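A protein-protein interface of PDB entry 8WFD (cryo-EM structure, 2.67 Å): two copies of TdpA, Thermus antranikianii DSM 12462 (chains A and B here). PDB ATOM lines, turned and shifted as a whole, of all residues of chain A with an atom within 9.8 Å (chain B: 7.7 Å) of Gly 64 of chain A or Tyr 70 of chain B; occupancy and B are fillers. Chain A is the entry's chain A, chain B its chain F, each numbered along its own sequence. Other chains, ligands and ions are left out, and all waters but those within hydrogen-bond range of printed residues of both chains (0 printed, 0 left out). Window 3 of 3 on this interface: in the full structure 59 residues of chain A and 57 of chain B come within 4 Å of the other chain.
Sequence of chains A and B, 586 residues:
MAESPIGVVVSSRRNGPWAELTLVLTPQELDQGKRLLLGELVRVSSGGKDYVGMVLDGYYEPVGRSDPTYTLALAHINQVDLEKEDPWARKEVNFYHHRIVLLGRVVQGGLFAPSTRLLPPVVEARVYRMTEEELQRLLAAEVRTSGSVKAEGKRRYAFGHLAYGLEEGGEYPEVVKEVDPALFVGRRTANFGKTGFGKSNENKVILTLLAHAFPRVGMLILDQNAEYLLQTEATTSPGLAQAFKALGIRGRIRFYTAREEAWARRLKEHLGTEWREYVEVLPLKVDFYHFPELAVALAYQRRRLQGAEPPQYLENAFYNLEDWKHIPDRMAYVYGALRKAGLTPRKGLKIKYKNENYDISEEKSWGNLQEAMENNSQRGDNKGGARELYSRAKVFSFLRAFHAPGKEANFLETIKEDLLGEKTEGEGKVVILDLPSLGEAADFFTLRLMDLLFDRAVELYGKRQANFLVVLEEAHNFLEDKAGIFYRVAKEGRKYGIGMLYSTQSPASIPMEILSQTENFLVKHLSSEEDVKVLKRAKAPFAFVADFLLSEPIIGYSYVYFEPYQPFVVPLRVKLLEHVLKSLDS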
ATOM      1  N   VAL A   8      17.996 -12.350  24.469  1.00  0.00           N
ATOM      2  CA  VAL A   8      17.169 -12.585  25.645  1.00  0.00           C
ATOM      3  C   VAL A   8      17.782 -11.833  26.818  1.00  0.00           C
ATOM      4  O   VAL A   8      18.994 -11.902  27.040  1.00  0.00           O
ATOM      5  CB  VAL A   8      17.033 -14.088  25.961  1.00  0.00           C
ATOM      6  CG1 VAL A   8      18.397 -14.730  26.127  1.00  0.00           C
ATOM      7  CG2 VAL A   8      16.185 -14.300  27.195  1.00  0.00           C
ATOM      8  N   VAL A   9      16.949 -11.107  27.558  1.00  0.00           N
ATOM      9  CA  VAL A   9      17.399 -10.389  28.746  1.00  0.00           C
ATOM     10  C   VAL A   9      17.457 -11.361  29.915  1.00  0.00           C
ATOM     11  O   VAL A   9      16.481 -12.060  30.205  1.00  0.00           O
ATOM     12  CB  VAL A   9      16.467  -9.205  29.052  1.00  0.00           C
ATOM     13  CG1 VAL A   9      16.883  -8.522  30.340  1.00  0.00           C
ATOM     14  CG2 VAL A   9      16.463  -8.220  27.902  1.00  0.00           C
ATOM     15  N   VAL A  10      18.601 -11.407  30.593  1.00  0.00           N
ATOM     16  CA  VAL A  10      18.821 -12.364  31.671  1.00  0.00           C
ATOM     17  C   VAL A  10      19.073 -11.705  33.019  1.00  0.00           C
ATOM     18  O   VAL A  10      19.172 -12.421  34.026  1.00  0.00           O
ATOM     19  CB  VAL A  10      19.976 -13.333  31.338  1.00  0.00           C
ATOM     20  CG1 VAL A  10      19.676 -14.095  30.061  1.00  0.00           C
ATOM     21  CG2 VAL A  10      21.283 -12.579  31.216  1.00  0.00           C
ATOM     22  N   SER A  11      19.178 -10.381  33.086  1.00  0.00           N
ATOM     23  CA  SER A  11      19.426  -9.710  34.353  1.00  0.00           C
ATOM     24  C   SER A  11      19.258  -8.211  34.165  1.00  0.00           C
ATOM     25  O   SER A  11      19.414  -7.689  33.062  1.00  0.00           O
ATOM     26  CB  SER A  11      20.823 -10.028  34.890  1.00  0.00           C
ATOM     27  OG  SER A  11      20.986  -9.546  36.210  1.00  0.00           O
ATOM     28  N   VAL A  24      21.880 -11.662  26.156  1.00  0.00           N
ATOM     29  CA  VAL A  24      22.613 -12.842  25.718  1.00  0.00           C
ATOM     30  C   VAL A  24      22.235 -13.140  24.275  1.00  0.00           C
ATOM     31  O   VAL A  24      21.048 -13.223  23.942  1.00  0.00           O
ATOM     32  CB  VAL A  24      22.330 -14.055  26.625  1.00  0.00           C
ATOM     33  CG1 VAL A  24      23.073 -15.278  26.125  1.00  0.00           C
ATOM     34  CG2 VAL A  24      22.728 -13.745  28.053  1.00  0.00           C
ATOM     35  N   THR A  26      22.454 -15.905  21.284  1.00  0.00           N
ATOM     36  CA  THR A  26      22.440 -17.356  21.224  1.00  0.00           C
ATOM     37  C   THR A  26      23.104 -17.863  19.952  1.00  0.00           C
ATOM     38  O   THR A  26      23.371 -17.096  19.021  1.00  0.00           O
ATOM     39  CB  THR A  26      21.004 -17.868  21.298  1.00  0.00           C
ATOM     40  OG1 THR A  26      20.300 -17.495  20.109  1.00  0.00           O
ATOM     41  CG2 THR A  26      20.292 -17.281  22.505  1.00  0.00           C
ATOM     42  N   PRO A  27      23.398 -19.166  19.899  1.00  0.00           N
ATOM     43  CA  PRO A  27      24.109 -19.706  18.729  1.00  0.00           C
ATOM     44  C   PRO A  27      23.399 -19.461  17.411  1.00  0.00           C
ATOM     45  O   PRO A  27      24.059 -19.165  16.410  1.00  0.00           O
ATOM     46  CB  PRO A  27      24.207 -21.203  19.050  1.00  0.00           C
ATOM     47  CG  PRO A  27      24.126 -21.276  20.530  1.00  0.00           C
ATOM     48  CD  PRO A  27      23.200 -20.180  20.944  1.00  0.00           C
ATOM     49  N   TYR A  60      32.606 -12.561  26.698  1.00  0.00           N
ATOM     50  CA  TYR A  60      32.263 -13.969  26.566  1.00  0.00           C
ATOM     51  C   TYR A  60      32.179 -14.605  27.944  1.00  0.00           C
ATOM     52  O   TYR A  60      33.086 -14.442  28.766  1.00  0.00           O
ATOM     53  CB  TYR A  60      33.291 -14.708  25.710  1.00  0.00           C
ATOM     54  CG  TYR A  60      32.992 -16.178  25.555  1.00  0.00           C
ATOM     55  CD1 TYR A  60      31.973 -16.613  24.725  1.00  0.00           C
ATOM     56  CD2 TYR A  60      33.724 -17.131  26.246  1.00  0.00           C
ATOM     57  CE1 TYR A  60      31.694 -17.952  24.584  1.00  0.00           C
ATOM     58  CE2 TYR A  60      33.451 -18.473  26.111  1.00  0.00           C
ATOM     59  CZ  TYR A  60      32.435 -18.877  25.278  1.00  0.00           C
ATOM     60  OH  TYR A  60      32.156 -20.215  25.136  1.00  0.00           O
ATOM     61  N   GLU A  61      31.093 -15.327  28.194  1.00  0.00           N
ATOM     62  CA  GLU A  61      30.883 -16.014  29.456  1.00  0.00           C
ATOM     63  C   GLU A  61      30.259 -17.375  29.188  1.00  0.00           C
ATOM     64  O   GLU A  61      29.471 -17.525  28.246  1.00  0.00           O
ATOM     65  CB  GLU A  61      29.979 -15.197  30.390  1.00  0.00           C
ATOM     66  CG  GLU A  61      29.466 -15.952  31.591  1.00  0.00           C
ATOM     67  CD  GLU A  61      29.171 -15.036  32.756  1.00  0.00           C
ATOM     68  OE1 GLU A  61      29.902 -14.037  32.923  1.00  0.00           O
ATOM     69  OE2 GLU A  61      28.211 -15.308  33.504  1.00  0.00           O
ATOM     70  N   PRO A  62      30.598 -18.383  29.988  1.00  0.00           N
ATOM     71  CA  PRO A  62      29.990 -19.706  29.803  1.00  0.00           C
ATOM     72  C   PRO A  62      28.543 -19.727  30.265  1.00  0.00           C
ATOM     73  O   PRO A  62      28.179 -19.103  31.264  1.00  0.00           O
ATOM     74  CB  PRO A  62      30.867 -20.625  30.665  1.00  0.00           C
ATOM     75  CG  PRO A  62      32.121 -19.843  30.925  1.00  0.00           C
ATOM     76  CD  PRO A  62      31.694 -18.415  30.968  1.00  0.00           C
ATOM     77  N   VAL A  63      27.715 -20.460  29.526  1.00  0.00           N
ATOM     78  CA  VAL A  63      26.293 -20.600  29.817  1.00  0.00           C
ATOM     79  C   VAL A  63      26.025 -22.045  30.214  1.00  0.00           C
ATOM     80  O   VAL A  63      26.409 -22.975  29.495  1.00  0.00           O
ATOM     81  CB  VAL A  63      25.425 -20.192  28.613  1.00  0.00           C
ATOM     82  CG1 VAL A  63      24.015 -20.723  28.775  1.00  0.00           C
ATOM     83  CG2 VAL A  63      25.408 -18.683  28.461  1.00  0.00           C
ATOM     84  N   GLY A  64      25.366 -22.231  31.352  1.00  0.00           N
ATOM     85  CA  GLY A  64      25.098 -23.566  31.841  1.00  0.00           C
ATOM     86  C   GLY A  64      26.319 -24.187  32.496  1.00  0.00           C
ATOM     87  O   GLY A  64      27.236 -23.503  32.961  1.00  0.00           O
ATOM     88  N   ARG A  65      26.321 -25.519  32.534  1.00  0.00           N
ATOM     89  CA  ARG A  65      27.428 -26.282  33.109  1.00  0.00           C
ATOM     90  C   ARG A  65      28.287 -26.807  31.963  1.00  0.00           C
ATOM     91  O   ARG A  65      28.135 -27.934  31.493  1.00  0.00           O
ATOM     92  CB  ARG A  65      26.900 -27.406  33.996  1.00  0.00           C
ATOM     93  CG  ARG A  65      26.701 -26.997  35.448  1.00  0.00           C
ATOM     94  CD  ARG A  65      25.921 -28.044  36.220  1.00  0.00           C
ATOM     95  NE  ARG A  65      24.494 -27.748  36.255  1.00  0.00           N
ATOM     96  CZ  ARG A  65      23.536 -28.655  36.122  1.00  0.00           C
ATOM     97  NH1 ARG A  65      23.818 -29.934  35.935  1.00  0.00           N
ATOM     98  NH2 ARG A  65      22.265 -28.270  36.175  1.00  0.00           N
ATOM     99  N   SER A  66      29.210 -25.962  31.510  1.00  0.00           N
ATOM    100  CA  SER A  66      30.049 -26.277  30.365  1.00  0.00           C
ATOM    101  C   SER A  66      31.457 -25.752  30.604  1.00  0.00           C
ATOM    102  O   SER A  66      31.684 -24.877  31.441  1.00  0.00           O
ATOM    103  CB  SER A  66      29.479 -25.688  29.067  1.00  0.00           C
ATOM    104  OG  SER A  66      29.651 -24.283  29.021  1.00  0.00           O
ATOM    105  N   ASP A  67      32.407 -26.308  29.849  1.00  0.00           N
ATOM    106  CA  ASP A  67      33.816 -25.918  29.903  1.00  0.00           C
ATOM    107  C   ASP A  67      34.252 -25.551  28.491  1.00  0.00           C
ATOM    108  O   ASP A  67      34.799 -26.394  27.757  1.00  0.00           O
ATOM    109  CB  ASP A  67      34.676 -27.039  30.480  1.00  0.00           C
ATOM    110  CG  ASP A  67      36.051 -26.562  30.904  1.00  0.00           C
ATOM    111  OD1 ASP A  67      36.422 -25.421  30.561  1.00  0.00           O
ATOM    112  OD2 ASP A  67      36.761 -27.329  31.583  1.00  0.00           O
ATOM    113  N   PRO A  68      34.011 -24.311  28.059  1.00  0.00           N
ATOM    114  CA  PRO A  68      34.365 -23.939  26.681  1.00  0.00           C
ATOM    115  C   PRO A  68      35.838 -24.111  26.372  1.00  0.00           C
ATOM    116  O   PRO A  68      36.186 -24.527  25.262  1.00  0.00           O
ATOM    117  CB  PRO A  68      33.933 -22.468  26.599  1.00  0.00           C
ATOM    118  CG  PRO A  68      32.924 -22.305  27.687  1.00  0.00           C
ATOM    119  CD  PRO A  68      33.398 -23.192  28.790  1.00  0.00           C
ATOM    120  N   LYS A  91      26.993 -25.767  19.610  1.00  0.00           N
ATOM    121  CA  LYS A  91      25.802 -25.071  20.078  1.00  0.00           C
ATOM    122  C   LYS A  91      25.842 -24.749  21.561  1.00  0.00           C
ATOM    123  O   LYS A  91      25.045 -23.926  22.023  1.00  0.00           O
ATOM    124  CB  LYS A  91      24.549 -25.904  19.795  1.00  0.00           C
ATOM    125  CG  LYS A  91      24.122 -25.926  18.345  1.00  0.00           C
ATOM    126  CD  LYS A  91      22.965 -26.885  18.142  1.00  0.00           C
ATOM    127  CE  LYS A  91      22.698 -27.118  16.668  1.00  0.00           C
ATOM    128  NZ  LYS A  91      21.706 -28.205  16.456  1.00  0.00           N
ATOM    129  N   GLU A  92      26.735 -25.378  22.317  1.00  0.00           N
ATOM    130  CA  GLU A  92      26.814 -25.171  23.755  1.00  0.00           C
ATOM    131  C   GLU A  92      27.891 -24.174  24.153  1.00  0.00           C
ATOM    132  O   GLU A  92      28.015 -23.860  25.340  1.00  0.00           O
ATOM    133  CB  GLU A  92      27.055 -26.505  24.464  1.00  0.00           C
ATOM    134  CG  GLU A  92      28.444 -27.071  24.257  1.00  0.00           C
ATOM    135  CD  GLU A  92      28.869 -27.979  25.389  1.00  0.00           C
ATOM    136  OE1 GLU A  92      28.195 -27.973  26.440  1.00  0.00           O
ATOM    137  OE2 GLU A  92      29.878 -28.698  25.229  1.00  0.00           O
ATOM    138  N   VAL A  93      28.671 -23.672  23.200  1.00  0.00           N
ATOM    139  CA  VAL A  93      29.714 -22.694  23.487  1.00  0.00           C
ATOM    140  C   VAL A  93      29.517 -21.381  22.748  1.00  0.00           C
ATOM    141  O   VAL A  93      30.244 -20.418  23.034  1.00  0.00           O
ATOM    142  CB  VAL A  93      31.118 -23.260  23.183  1.00  0.00           C
ATOM    143  CG1 VAL A  93      31.511 -24.297  24.217  1.00  0.00           C
ATOM    144  CG2 VAL A  93      31.166 -23.850  21.788  1.00  0.00           C
ATOM    145  N   PHE A  95      27.743 -18.498  22.635  1.00  0.00           N
ATOM    146  CA  PHE A  95      26.914 -17.499  23.294  1.00  0.00           C
ATOM    147  C   PHE A  95      27.736 -16.229  23.457  1.00  0.00           C
ATOM    148  O   PHE A  95      28.967 -16.270  23.448  1.00  0.00           O
ATOM    149  CB  PHE A  95      26.432 -17.979  24.669  1.00  0.00           C
ATOM    150  CG  PHE A  95      25.422 -19.086  24.612  1.00  0.00           C
ATOM    151  CD1 PHE A  95      24.069 -18.807  24.541  1.00  0.00           C
ATOM    152  CD2 PHE A  95      25.827 -20.408  24.641  1.00  0.00           C
ATOM    153  CE1 PHE A  95      23.144 -19.825  24.495  1.00  0.00           C
ATOM    154  CE2 PHE A  95      24.906 -21.427  24.594  1.00  0.00           C
ATOM    155  CZ  PHE A  95      23.563 -21.136  24.521  1.00  0.00           C
ATOM    156  N   HIS A  97      27.654 -12.080  25.506  1.00  0.00           N
ATOM    157  CA  HIS A  97      27.011 -11.231  26.502  1.00  0.00           C
ATOM    158  C   HIS A  97      27.202  -9.755  26.172  1.00  0.00           C
ATOM    159  O   HIS A  97      28.245  -9.346  25.658  1.00  0.00           O
ATOM    160  CB  HIS A  97      27.564 -11.505  27.904  1.00  0.00           C
ATOM    161  CG  HIS A  97      26.988 -12.722  28.559  1.00  0.00           C
ATOM    162  ND1 HIS A  97      27.122 -13.987  28.031  1.00  0.00           N
ATOM    163  CD2 HIS A  97      26.283 -12.866  29.704  1.00  0.00           C
ATOM    164  CE1 HIS A  97      26.522 -14.857  28.821  1.00  0.00           C
ATOM    165  NE2 HIS A  97      26.005 -14.203  29.844  1.00  0.00           N
ATOM    166  N   SER B  66      18.522 -22.464  41.007  1.00  0.00           N
ATOM    167  CA  SER B  66      18.045 -22.201  39.658  1.00  0.00           C
ATOM    168  C   SER B  66      19.161 -21.567  38.841  1.00  0.00           C
ATOM    169  O   SER B  66      20.108 -20.995  39.385  1.00  0.00           O
ATOM    170  CB  SER B  66      16.808 -21.298  39.666  1.00  0.00           C
ATOM    171  OG  SER B  66      17.053 -20.098  40.376  1.00  0.00           O
ATOM    172  N   ASP B  67      19.028 -21.680  37.520  1.00  0.00           N
ATOM    173  CA  ASP B  67      19.948 -21.068  36.563  1.00  0.00           C
ATOM    174  C   ASP B  67      19.114 -20.231  35.604  1.00  0.00           C
ATOM    175  O   ASP B  67      18.737 -20.696  34.517  1.00  0.00           O
ATOM    176  CB  ASP B  67      20.766 -22.119  35.820  1.00  0.00           C
ATOM    177  CG  ASP B  67      21.942 -21.521  35.075  1.00  0.00           C
ATOM    178  OD1 ASP B  67      22.249 -20.332  35.294  1.00  0.00           O
ATOM    179  OD2 ASP B  67      22.563 -22.242  34.268  1.00  0.00           O
ATOM    180  N   PRO B  68      18.789 -18.993  35.982  1.00  0.00           N
ATOM    181  CA  PRO B  68      17.922 -18.174  35.121  1.00  0.00           C
ATOM    182  C   PRO B  68      18.482 -17.975  33.729  1.00  0.00           C
ATOM    183  O   PRO B  68      17.722 -17.987  32.754  1.00  0.00           O
ATOM    184  CB  PRO B  68      17.819 -16.850  35.890  1.00  0.00           C
ATOM    185  CG  PRO B  68      18.205 -17.180  37.289  1.00  0.00           C
ATOM    186  CD  PRO B  68      19.219 -18.265  37.185  1.00  0.00           C
ATOM    187  N   THR B  69      19.797 -17.792  33.606  1.00  0.00           N
ATOM    188  CA  THR B  69      20.385 -17.588  32.288  1.00  0.00           C
ATOM    189  C   THR B  69      20.138 -18.789  31.391  1.00  0.00           C
ATOM    190  O   THR B  69      19.659 -18.640  30.261  1.00  0.00           O
ATOM    191  CB  THR B  69      21.884 -17.316  32.414  1.00  0.00           C
ATOM    192  OG1 THR B  69      22.115 -16.393  33.484  1.00  0.00           O
ATOM    193  CG2 THR B  69      22.427 -16.731  31.122  1.00  0.00           C
ATOM    194  N   TYR B  70      20.442 -19.992  31.881  1.00  0.00           N
ATOM    195  CA  TYR B  70      20.230 -21.188  31.074  1.00  0.00           C
ATOM    196  C   TYR B  70      18.756 -21.387  30.754  1.00  0.00           C
ATOM    197  O   TYR B  70      18.404 -21.698  29.612  1.00  0.00           O
ATOM    198  CB  TYR B  70      20.792 -22.416  31.787  1.00  0.00           C
ATOM    199  CG  TYR B  70      20.819 -23.648  30.916  1.00  0.00           C
ATOM    200  CD1 TYR B  70      21.758 -23.788  29.906  1.00  0.00           C
ATOM    201  CD2 TYR B  70      19.896 -24.669  31.095  1.00  0.00           C
ATOM    202  CE1 TYR B  70      21.781 -24.908  29.103  1.00  0.00           C
ATOM    203  CE2 TYR B  70      19.912 -25.793  30.299  1.00  0.00           C
ATOM    204  CZ  TYR B  70      20.856 -25.907  29.304  1.00  0.00           C
ATOM    205  OH  TYR B  70      20.878 -27.028  28.506  1.00  0.00           O
ATOM    206  N   THR B  71      17.876 -21.204  31.740  1.00  0.00           N
ATOM    207  CA  THR B  71      16.454 -21.422  31.489  1.00  0.00           C
ATOM    208  C   THR B  71      15.919 -20.460  30.434  1.00  0.00           C
ATOM    209  O   THR B  71      15.244 -20.880  29.484  1.00  0.00           O
ATOM    210  CB  THR B  71      15.667 -21.284  32.792  1.00  0.00           C
ATOM    211  OG1 THR B  71      16.070 -22.313  33.704  1.00  0.00           O
ATOM    212  CG2 THR B  71      14.178 -21.405  32.531  1.00  0.00           C
ATOM    213  N   LEU B  72      16.221 -19.167  30.574  1.00  0.00           N
ATOM    214  CA  LEU B  72      15.708 -18.179  29.633  1.00  0.00           C
ATOM    215  C   LEU B  72      16.329 -18.351  28.252  1.00  0.00           C
ATOM    216  O   LEU B  72      15.639 -18.207  27.236  1.00  0.00           O
ATOM    217  CB  LEU B  72      15.955 -16.770  30.171  1.00  0.00           C
ATOM    218  CG  LEU B  72      15.146 -16.383  31.411  1.00  0.00           C
ATOM    219  CD1 LEU B  72      15.796 -15.227  32.149  1.00  0.00           C
ATOM    220  CD2 LEU B  72      13.715 -16.041  31.041  1.00  0.00           C
ATOM    221  N   ALA B  73      17.626 -18.664  28.188  1.00  0.00           N
ATOM    222  CA  ALA B  73      18.265 -18.887  26.897  1.00  0.00           C
ATOM    223  C   ALA B  73      17.682 -20.107  26.200  1.00  0.00           C
ATOM    224  O   ALA B  73      17.478 -20.094  24.982  1.00  0.00           O
ATOM    225  CB  ALA B  73      19.774 -19.037  27.074  1.00  0.00           C
ATOM    226  N   LEU B  74      17.412 -21.176  26.951  1.00  0.00           N
ATOM    227  CA  LEU B  74      16.814 -22.365  26.353  1.00  0.00           C
ATOM    228  C   LEU B  74      15.409 -22.076  25.845  1.00  0.00           C
ATOM    229  O   LEU B  74      15.033 -22.511  24.749  1.00  0.00           O
ATOM    230  CB  LEU B  74      16.799 -23.501  27.375  1.00  0.00           C
ATOM    231  CG  LEU B  74      16.663 -24.924  26.844  1.00  0.00           C
ATOM    232  CD1 LEU B  74      17.888 -25.294  26.029  1.00  0.00           C
ATOM    233  CD2 LEU B  74      16.467 -25.897  27.991  1.00  0.00           C
ATOM    234  N   ALA B  75      14.615 -21.341  26.628  1.00  0.00           N
ATOM    235  CA  ALA B  75      13.282 -20.968  26.168  1.00  0.00           C
ATOM    236  C   ALA B  75      13.353 -20.126  24.900  1.00  0.00           C
ATOM    237  O   ALA B  75      12.571 -20.329  23.967  1.00  0.00           O
ATOM    238  CB  ALA B  75      12.535 -20.221  27.271  1.00  0.00           C
ATOM    239  N   HIS B  76      14.288 -19.175  24.848  1.00  0.00           N
ATOM    240  CA  HIS B  76      14.444 -18.356  23.650  1.00  0.00           C
ATOM    241  C   HIS B  76      14.866 -19.200  22.454  1.00  0.00           C
ATOM    242  O   HIS B  76      14.362 -19.009  21.341  1.00  0.00           O
ATOM    243  CB  HIS B  76      15.461 -17.245  23.908  1.00  0.00           C
ATOM    244  CG  HIS B  76      15.614 -16.284  22.772  1.00  0.00           C
ATOM    245  ND1 HIS B  76      14.647 -15.360  22.444  1.00  0.00           N
ATOM    246  CD2 HIS B  76      16.624 -16.100  21.889  1.00  0.00           C
ATOM    247  CE1 HIS B  76      15.052 -14.651  21.406  1.00  0.00           C
ATOM    248  NE2 HIS B  76      16.249 -15.081  21.049  1.00  0.00           N
ATOM    249  N   ILE B  77      15.796 -20.131  22.663  1.00  0.00           N
ATOM    250  CA  ILE B  77      16.277 -20.972  21.571  1.00  0.00           C
ATOM    251  C   ILE B  77      15.139 -21.809  21.006  1.00  0.00           C
ATOM    252  O   ILE B  77      14.950 -21.892  19.788  1.00  0.00           O
ATOM    253  CB  ILE B  77      17.441 -21.856  22.051  1.00  0.00           C
ATOM    254  CG1 ILE B  77      18.729 -21.035  22.155  1.00  0.00           C
ATOM    255  CG2 ILE B  77      17.623 -23.045  21.126  1.00  0.00           C
ATOM    256  CD1 ILE B  77      19.834 -21.727  22.915  1.00  0.00           C
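Leu 72 of chain B touches Val 8 of chain A (CB to CG2, 3.9 Å). Val 9 of chain A touches Leu 72 of chain B (O to CD1, 3.8 Å). Thr 69 of chain B touches Val 10 of chain A. CG2 of Thr 26 of chain A touches CD2 of His 76 of chain B (3.9 Å). Thr 26 of chain A touches Ile 77 of chain B (CB to CG1, 3.99 Å). Val 63 of chain A touches Tyr 70 of chain B. Gly 64 of chain A touches Asp 67 of chain B (CA to OD2, 3.8 Å). CA of Gly 64 of chain A touches CD1 of Tyr 70 of chain B, 3.9 Å away.
Of the 12 printed residues of chain B, 6 touch a printed residue of chain A. Hydrophobic or aromatic side chains of chain B within 4 Å of the printed part of chain A: Tyr 70, Leu 72, His 76 and Ile 77. Of the 21 printed residues of chain A, 6 touch a printed residue of chain B. Printed residues of chain A that touch a printed residue of chain B: Val 8, Val 9, Val 10, Thr 26, Val 63 and Gly 64. Hydrophobic or aromatic side chains of chain A within 4 Å of the printed part of chain B: Val 8, Val 10 and Val 63. Among the printed residues, 8 pairs touch across the chains. Among the printed residues, no Asp or Glu carboxylate lies within 4 Å of a Lys or Arg side-chain nitrogen of the other chain.
OG1 of Thr 71 of chain B sits at hydrogen-bond distance from O of Asp 67 of chain B (3.2 Å). The backbone NH of Val 24 of chain A is in hydrogen-bond range of the backbone carbonyl oxygen of Val 8 of chain A.
Of the printed residues of chain B, Val 8 of chain A touches Leu 72. Printed residues of chain B within 4 Å of Thr 26 of chain A: His 76 and Ile 77. Gly 64 of chain A touches just these residues of chain B: Asp 67 (3.8 Å) and Tyr 70 (3.9 Å). Ser 66 of chain B touches none of the printed residues of chain A. Printed residues of chain A within 4 Å of Asp 67 of chain B: Gly 64 (3.8 Å). Tyr 70 of chain B touches two residues of chain A. No residue of chain A comes within 4 Å of Thr 71 of chain B. Of the printed residues of chain A, Leu 72 of chain B touches Val 8 and Val 9. No residue of chain A comes within 4 Å of Ala 73 of chain B. Printed residues of chain A within 4 Å of Ile 77 of chain B: Thr 26 (3.99 Å). The nearest residue of chain A that does not touch Tyr 70 of chain B is Arg 65 of chain A (5.5 Å).
3 positions are printed for both chains. Of the 8 pairs that touch across the chains among the printed residues, none has its exchanged pair printed and touching as well.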
